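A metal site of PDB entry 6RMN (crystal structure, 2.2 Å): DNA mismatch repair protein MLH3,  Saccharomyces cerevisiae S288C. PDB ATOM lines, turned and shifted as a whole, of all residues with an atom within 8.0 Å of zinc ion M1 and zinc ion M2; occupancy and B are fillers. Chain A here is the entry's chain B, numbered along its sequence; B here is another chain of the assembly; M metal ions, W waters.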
ATOM      1  N   ASP A  47      11.265  11.283 -31.696  1.00  0.00           N
ATOM      2  CA  ASP A  47      11.324  10.207 -30.705  1.00  0.00           C
ATOM      3  C   ASP A  47       9.981   9.434 -30.850  1.00  0.00           C
ATOM      4  O   ASP A  47       8.913  10.029 -30.719  1.00  0.00           O
ATOM      5  CB  ASP A  47      11.451  10.835 -29.300  1.00  0.00           C
ATOM      6  CG  ASP A  47      11.501   9.886 -28.100  1.00  0.00           C
ATOM      7  OD1 ASP A  47      10.891   8.796 -28.170  1.00  0.00           O
ATOM      8  OD2 ASP A  47      12.115  10.259 -27.080  1.00  0.00           O
ATOM      9  N   HIS A  49       8.611   7.152 -28.955  1.00  0.00           N
ATOM     10  CA  HIS A  49       7.916   7.005 -27.682  1.00  0.00           C
ATOM     11  C   HIS A  49       7.197   8.313 -27.316  1.00  0.00           C
ATOM     12  O   HIS A  49       5.997   8.268 -27.029  1.00  0.00           O
ATOM     13  CB  HIS A  49       8.894   6.551 -26.578  1.00  0.00           C
ATOM     14  CG  HIS A  49       8.263   6.529 -25.232  1.00  0.00           C
ATOM     15  ND1 HIS A  49       7.345   5.559 -24.873  1.00  0.00           N
ATOM     16  CD2 HIS A  49       8.370   7.413 -24.217  1.00  0.00           C
ATOM     17  CE1 HIS A  49       6.960   5.863 -23.651  1.00  0.00           C
ATOM     18  NE2 HIS A  49       7.554   6.957 -23.219  1.00  0.00           N
ATOM     19  N   ALA A  50       7.910   9.449 -27.371  1.00  0.00           N
ATOM     20  CA  ALA A  50       7.397  10.797 -27.082  1.00  0.00           C
ATOM     21  C   ALA A  50       6.216  11.143 -27.988  1.00  0.00           C
ATOM     22  O   ALA A  50       5.227  11.694 -27.519  1.00  0.00           O
ATOM     23  CB  ALA A  50       8.500  11.828 -27.243  1.00  0.00           C
ATOM     24  N   GLU A  53       3.216   8.826 -26.880  1.00  0.00           N
ATOM     25  CA  GLU A  53       2.826   9.310 -25.550  1.00  0.00           C
ATOM     26  C   GLU A  53       2.051  10.625 -25.648  1.00  0.00           C
ATOM     27  O   GLU A  53       1.047  10.780 -24.958  1.00  0.00           O
ATOM     28  CB  GLU A  53       4.074   9.479 -24.671  1.00  0.00           C
ATOM     29  CG  GLU A  53       3.824   9.913 -23.246  1.00  0.00           C
ATOM     30  CD  GLU A  53       5.124  10.069 -22.498  1.00  0.00           C
ATOM     31  OE1 GLU A  53       5.760   9.032 -22.197  1.00  0.00           O
ATOM     32  OE2 GLU A  53       5.541  11.218 -22.269  1.00  0.00           O
ATOM     33  N   ARG A  54       2.482  11.544 -26.541  1.00  0.00           N
ATOM     34  CA  ARG A  54       1.835  12.828 -26.787  1.00  0.00           C
ATOM     35  C   ARG A  54       0.401  12.654 -27.342  1.00  0.00           C
ATOM     36  O   ARG A  54      -0.532  13.312 -26.854  1.00  0.00           O
ATOM     37  CB  ARG A  54       2.658  13.684 -27.753  1.00  0.00           C
ATOM     38  CG  ARG A  54       2.048  15.070 -27.987  1.00  0.00           C
ATOM     39  CD  ARG A  54       2.320  15.916 -26.779  1.00  0.00           C
ATOM     40  NE  ARG A  54       1.114  16.424 -26.168  1.00  0.00           N
ATOM     41  CZ  ARG A  54       1.101  17.225 -25.105  1.00  0.00           C
ATOM     42  NH1 ARG A  54       2.244  17.575 -24.521  1.00  0.00           N
ATOM     43  NH2 ARG A  54      -0.043  17.659 -24.617  1.00  0.00           N
ATOM     44  N   ASN A 190      -0.468  11.285 -17.374  1.00  0.00           N
ATOM     45  CA  ASN A 190       0.911  11.265 -17.868  1.00  0.00           C
ATOM     46  C   ASN A 190       1.487   9.875 -17.804  1.00  0.00           C
ATOM     47  O   ASN A 190       2.107   9.449 -18.791  1.00  0.00           O
ATOM     48  CB  ASN A 190       1.814  12.224 -17.099  1.00  0.00           C
ATOM     49  CG  ASN A 190       1.683  13.672 -17.512  1.00  0.00           C
ATOM     50  OD1 ASN A 190       0.884  14.018 -18.386  1.00  0.00           O
ATOM     51  ND2 ASN A 190       2.455  14.547 -16.867  1.00  0.00           N
ATOM     52  N   SER A 191       1.253   9.163 -16.688  1.00  0.00           N
ATOM     53  CA  SER A 191       1.758   7.808 -16.485  1.00  0.00           C
ATOM     54  C   SER A 191       1.018   6.753 -17.281  1.00  0.00           C
ATOM     55  O   SER A 191       1.653   5.773 -17.681  1.00  0.00           O
ATOM     56  CB  SER A 191       1.807   7.451 -15.003  1.00  0.00           C
ATOM     57  OG  SER A 191       0.508   7.318 -14.456  1.00  0.00           O
ATOM     58  N   ALA A 193      -0.394   7.299 -20.313  1.00  0.00           N
ATOM     59  CA  ALA A 193       0.042   7.588 -21.679  1.00  0.00           C
ATOM     60  C   ALA A 193       1.444   7.040 -21.914  1.00  0.00           C
ATOM     61  O   ALA A 193       1.659   6.362 -22.921  1.00  0.00           O
ATOM     62  CB  ALA A 193      -0.003   9.090 -21.945  1.00  0.00           C
ATOM     63  N   CYS A 194       2.366   7.270 -20.957  1.00  0.00           N
ATOM     64  CA  CYS A 194       3.743   6.774 -20.981  1.00  0.00           C
ATOM     65  C   CYS A 194       3.751   5.245 -21.094  1.00  0.00           C
ATOM     66  O   CYS A 194       4.382   4.704 -22.012  1.00  0.00           O
ATOM     67  CB  CYS A 194       4.503   7.252 -19.744  1.00  0.00           C
ATOM     68  SG  CYS A 194       6.261   6.816 -19.742  1.00  0.00           S
ATOM     69  N   ARG A 195       2.981   4.564 -20.229  1.00  0.00           N
ATOM     70  CA  ARG A 195       2.865   3.106 -20.202  1.00  0.00           C
ATOM     71  C   ARG A 195       2.258   2.478 -21.434  1.00  0.00           C
ATOM     72  O   ARG A 195       2.625   1.363 -21.767  1.00  0.00           O
ATOM     73  CB  ARG A 195       2.070   2.652 -18.971  1.00  0.00           C
ATOM     74  CG  ARG A 195       2.906   2.602 -17.732  1.00  0.00           C
ATOM     75  CD  ARG A 195       3.462   1.233 -17.424  1.00  0.00           C
ATOM     76  NE  ARG A 195       4.036   1.301 -16.083  1.00  0.00           N
ATOM     77  CZ  ARG A 195       3.418   0.900 -14.979  1.00  0.00           C
ATOM     78  NH1 ARG A 195       2.252   0.277 -15.043  1.00  0.00           N
ATOM     79  NH2 ARG A 195       4.004   1.079 -13.796  1.00  0.00           N
ATOM     80  N   SER A 196       1.280   3.146 -22.055  1.00  0.00           N
ATOM     81  CA  SER A 196       0.597   2.611 -23.231  1.00  0.00           C
ATOM     82  C   SER A 196       1.400   2.811 -24.505  1.00  0.00           C
ATOM     83  O   SER A 196       1.187   2.078 -25.471  1.00  0.00           O
ATOM     84  CB  SER A 196      -0.783   3.237 -23.366  1.00  0.00           C
ATOM     85  OG  SER A 196      -1.674   2.706 -22.415  1.00  0.00           O
ATOM     86  N   ALA A 197       2.299   3.815 -24.511  1.00  0.00           N
ATOM     87  CA  ALA A 197       3.108   4.204 -25.652  1.00  0.00           C
ATOM     88  C   ALA A 197       4.113   3.173 -26.078  1.00  0.00           C
ATOM     89  O   ALA A 197       4.601   2.384 -25.268  1.00  0.00           O
ATOM     90  CB  ALA A 197       3.801   5.539 -25.397  1.00  0.00           C
ATOM     91  N   VAL A 198       4.445   3.195 -27.386  1.00  0.00           N
ATOM     92  CA  VAL A 198       5.443   2.351 -28.022  1.00  0.00           C
ATOM     93  C   VAL A 198       6.801   2.721 -27.383  1.00  0.00           C
ATOM     94  O   VAL A 198       6.985   3.861 -26.962  1.00  0.00           O
ATOM     95  CB  VAL A 198       5.373   2.493 -29.580  1.00  0.00           C
ATOM     96  CG1 VAL A 198       5.969   3.798 -30.100  1.00  0.00           C
ATOM     97  CG2 VAL A 198       5.983   1.301 -30.282  1.00  0.00           C
ATOM     98  N   MET A 199       7.698   1.742 -27.231  1.00  0.00           N
ATOM     99  CA  MET A 199       8.992   1.967 -26.594  1.00  0.00           C
ATOM    100  C   MET A 199      10.176   1.975 -27.573  1.00  0.00           C
ATOM    101  O   MET A 199      10.034   1.570 -28.728  1.00  0.00           O
ATOM    102  CB  MET A 199       9.230   0.883 -25.523  1.00  0.00           C
ATOM    103  CG  MET A 199       8.702   1.228 -24.150  1.00  0.00           C
ATOM    104  SD  MET A 199       9.133  -0.033 -22.904  1.00  0.00           S
ATOM    105  CE  MET A 199      10.851   0.417 -22.545  1.00  0.00           C
ATOM    106  N   GLU A 224       6.502  18.334 -27.546  1.00  0.00           N
ATOM    107  CA  GLU A 224       7.018  17.705 -26.328  1.00  0.00           C
ATOM    108  C   GLU A 224       6.217  16.479 -25.952  1.00  0.00           C
ATOM    109  O   GLU A 224       5.105  16.327 -26.417  1.00  0.00           O
ATOM    110  CB  GLU A 224       7.153  18.708 -25.141  1.00  0.00           C
ATOM    111  CG  GLU A 224       5.890  19.382 -24.655  1.00  0.00           C
ATOM    112  CD  GLU A 224       6.124  20.597 -23.772  1.00  0.00           C
ATOM    113  OE1 GLU A 224       6.874  21.506 -24.199  1.00  0.00           O
ATOM    114  OE2 GLU A 224       5.545  20.653 -22.670  1.00  0.00           O
ATOM    115  N   CYS A 225       6.798  15.581 -25.151  1.00  0.00           N
ATOM    116  CA  CYS A 225       6.144  14.376 -24.627  1.00  0.00           C
ATOM    117  C   CYS A 225       5.175  14.816 -23.503  1.00  0.00           C
ATOM    118  O   CYS A 225       5.053  16.020 -23.209  1.00  0.00           O
ATOM    119  CB  CYS A 225       7.179  13.388 -24.110  1.00  0.00           C
ATOM    120  SG  CYS A 225       7.958  13.882 -22.555  1.00  0.00           S
ATOM    121  N   ALA A 226       4.512  13.835 -22.828  1.00  0.00           N
ATOM    122  CA  ALA A 226       3.611  14.142 -21.719  1.00  0.00           C
ATOM    123  C   ALA A 226       4.304  14.877 -20.545  1.00  0.00           C
ATOM    124  O   ALA A 226       3.675  15.740 -19.945  1.00  0.00           O
ATOM    125  CB  ALA A 226       2.920  12.886 -21.209  1.00  0.00           C
ATOM    126  N   HIS A 227       5.606  14.577 -20.283  1.00  0.00           N
ATOM    127  CA  HIS A 227       6.422  15.142 -19.191  1.00  0.00           C
ATOM    128  C   HIS A 227       7.239  16.391 -19.566  1.00  0.00           C
ATOM    129  O   HIS A 227       8.203  16.732 -18.878  1.00  0.00           O
ATOM    130  CB  HIS A 227       7.333  14.048 -18.599  1.00  0.00           C
ATOM    131  CG  HIS A 227       6.624  12.747 -18.365  1.00  0.00           C
ATOM    132  ND1 HIS A 227       6.462  11.824 -19.382  1.00  0.00           N
ATOM    133  CD2 HIS A 227       5.985  12.292 -17.257  1.00  0.00           C
ATOM    134  CE1 HIS A 227       5.748  10.842 -18.864  1.00  0.00           C
ATOM    135  NE2 HIS A 227       5.437  11.075 -17.591  1.00  0.00           N
ATOM    136  N   GLY A 228       6.835  17.090 -20.630  1.00  0.00           N
ATOM    137  CA  GLY A 228       7.461  18.322 -21.095  1.00  0.00           C
ATOM    138  C   GLY A 228       8.826  18.276 -21.768  1.00  0.00           C
ATOM    139  O   GLY A 228       9.395  19.331 -22.032  1.00  0.00           O
ATOM    140  N   ARG A 229       9.353  17.073 -22.066  1.00  0.00           N
ATOM    141  CA  ARG A 229      10.653  16.892 -22.744  1.00  0.00           C
ATOM    142  C   ARG A 229      10.464  16.952 -24.287  1.00  0.00           C
ATOM    143  O   ARG A 229       9.409  16.501 -24.751  1.00  0.00           O
ATOM    144  CB  ARG A 229      11.325  15.575 -22.310  1.00  0.00           C
ATOM    145  CG  ARG A 229      11.633  15.521 -20.827  1.00  0.00           C
ATOM    146  CD  ARG A 229      12.796  14.608 -20.521  1.00  0.00           C
ATOM    147  NE  ARG A 229      13.099  14.559 -19.088  1.00  0.00           N
ATOM    148  CZ  ARG A 229      14.061  15.260 -18.495  1.00  0.00           C
ATOM    149  NH1 ARG A 229      14.824  16.086 -19.197  1.00  0.00           N
ATOM    150  NH2 ARG A 229      14.264  15.140 -17.187  1.00  0.00           N
ATOM    151  N   PRO A 230      11.418  17.493 -25.091  1.00  0.00           N
ATOM    152  CA  PRO A 230      11.208  17.573 -26.559  1.00  0.00           C
ATOM    153  C   PRO A 230      10.916  16.243 -27.247  1.00  0.00           C
ATOM    154  O   PRO A 230      11.499  15.224 -26.873  1.00  0.00           O
ATOM    155  CB  PRO A 230      12.505  18.198 -27.079  1.00  0.00           C
ATOM    156  CG  PRO A 230      13.494  17.944 -26.011  1.00  0.00           C
ATOM    157  CD  PRO A 230      12.723  18.076 -24.732  1.00  0.00           C
ATOM    158  N   ARG B 264      15.989  10.320 -20.761  1.00  0.00           N
ATOM    159  CA  ARG B 264      14.901  10.023 -19.833  1.00  0.00           C
ATOM    160  C   ARG B 264      13.634  10.657 -20.392  1.00  0.00           C
ATOM    161  O   ARG B 264      13.730  11.599 -21.190  1.00  0.00           O
ATOM    162  CB  ARG B 264      15.230  10.519 -18.418  1.00  0.00           C
ATOM    163  CG  ARG B 264      16.317   9.711 -17.713  1.00  0.00           C
ATOM    164  CD  ARG B 264      16.348   9.989 -16.214  1.00  0.00           C
ATOM    165  NE  ARG B 264      17.258   9.088 -15.505  1.00  0.00           N
ATOM    166  CZ  ARG B 264      17.361   9.004 -14.183  1.00  0.00           C
ATOM    167  NH1 ARG B 264      18.217   8.156 -13.623  1.00  0.00           N
ATOM    168  NH2 ARG B 264      16.608   9.773 -13.399  1.00  0.00           N
ATOM    169  N   CYS B 265      12.464  10.122 -20.032  1.00  0.00           N
ATOM    170  CA  CYS B 265      11.174  10.630 -20.511  1.00  0.00           C
ATOM    171  C   CYS B 265      10.741  11.885 -19.738  1.00  0.00           C
ATOM    172  O   CYS B 265      11.273  12.139 -18.631  1.00  0.00           O
ATOM    173  CB  CYS B 265      10.100   9.541 -20.480  1.00  0.00           C
ATOM    174  SG  CYS B 265       8.631   9.903 -21.470  1.00  0.00           S
ATOM    175  OXT CYS B 265       9.895  12.654 -20.250  1.00  0.00           O
HETATM  176 ZN    ZN M   1       7.311   8.087 -21.422  1.00  0.00          ZN
HETATM  177 ZN    ZN M   2       7.579  11.833 -21.321  1.00  0.00          ZN
HETATM  178  O   HOH W   1       9.981   6.213 -20.884  1.00  0.00           O
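The side-chain sulfur (SG) of Cys 225 lies close to the backbone NH (N) of Arg 229 (3.5 Å). N of His 49 lies within hydrogen-bond range of OD1 of Asp 47 (2.9 Å). The backbone carbonyl oxygen of Cys 225 lies within hydrogen-bond range of the guanidinium group of Arg 54. ND1 of His 49 lies within hydrogen-bond range of O of Val 198 (2.7 Å). The side-chain carboxylate of Glu 53 lies close to the backbone NH of Ala 226, at 2.9 Å. O of Cys 265 of chain B is in salt-bridge range of NE of Arg 229, 3.1 Å away.
Along chain A the residues within 4 Å of zinc ion M1 span positions 49 to 194.
Residues that only touch zinc ion M2: Ala 226 (3.96 Å). Five residues have an atom within 4 Å of zinc ion M2: Glu 53, Cys 225, Ala 226, His 227 and Cys 265 of chain B.
Zinc ion M1 is bound by OE1 of Glu 53 (2.0 Å). A ring nitrogen (NE2) of His 49 binds zinc ion M1, at 2.1 Å. Zinc ion M1 is bound by SG of Cys 265 of chain B, at 2.2 Å. Zinc ion M1 is bound by SG of Cys 194, 2.4 Å away. Zinc ion M1 has four donor atoms within binding distance.
Zinc ion M2 is bound by SG of Cys 265 of chain B (2.2 Å). Zinc ion M2 is bound by ND1 of His 227 (2.2 Å). Zinc ion M2 is bound by OE2 of Glu 53, at 2.3 Å. SG of Cys 225 is bound to zinc ion M2, 2.4 Å away. Zinc ion M2 has four donor atoms within binding distance. Slightly farther from zinc ion M2 lies the chain-end carboxylate (OXT) of Cys 265 of chain B (2.7 Å).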
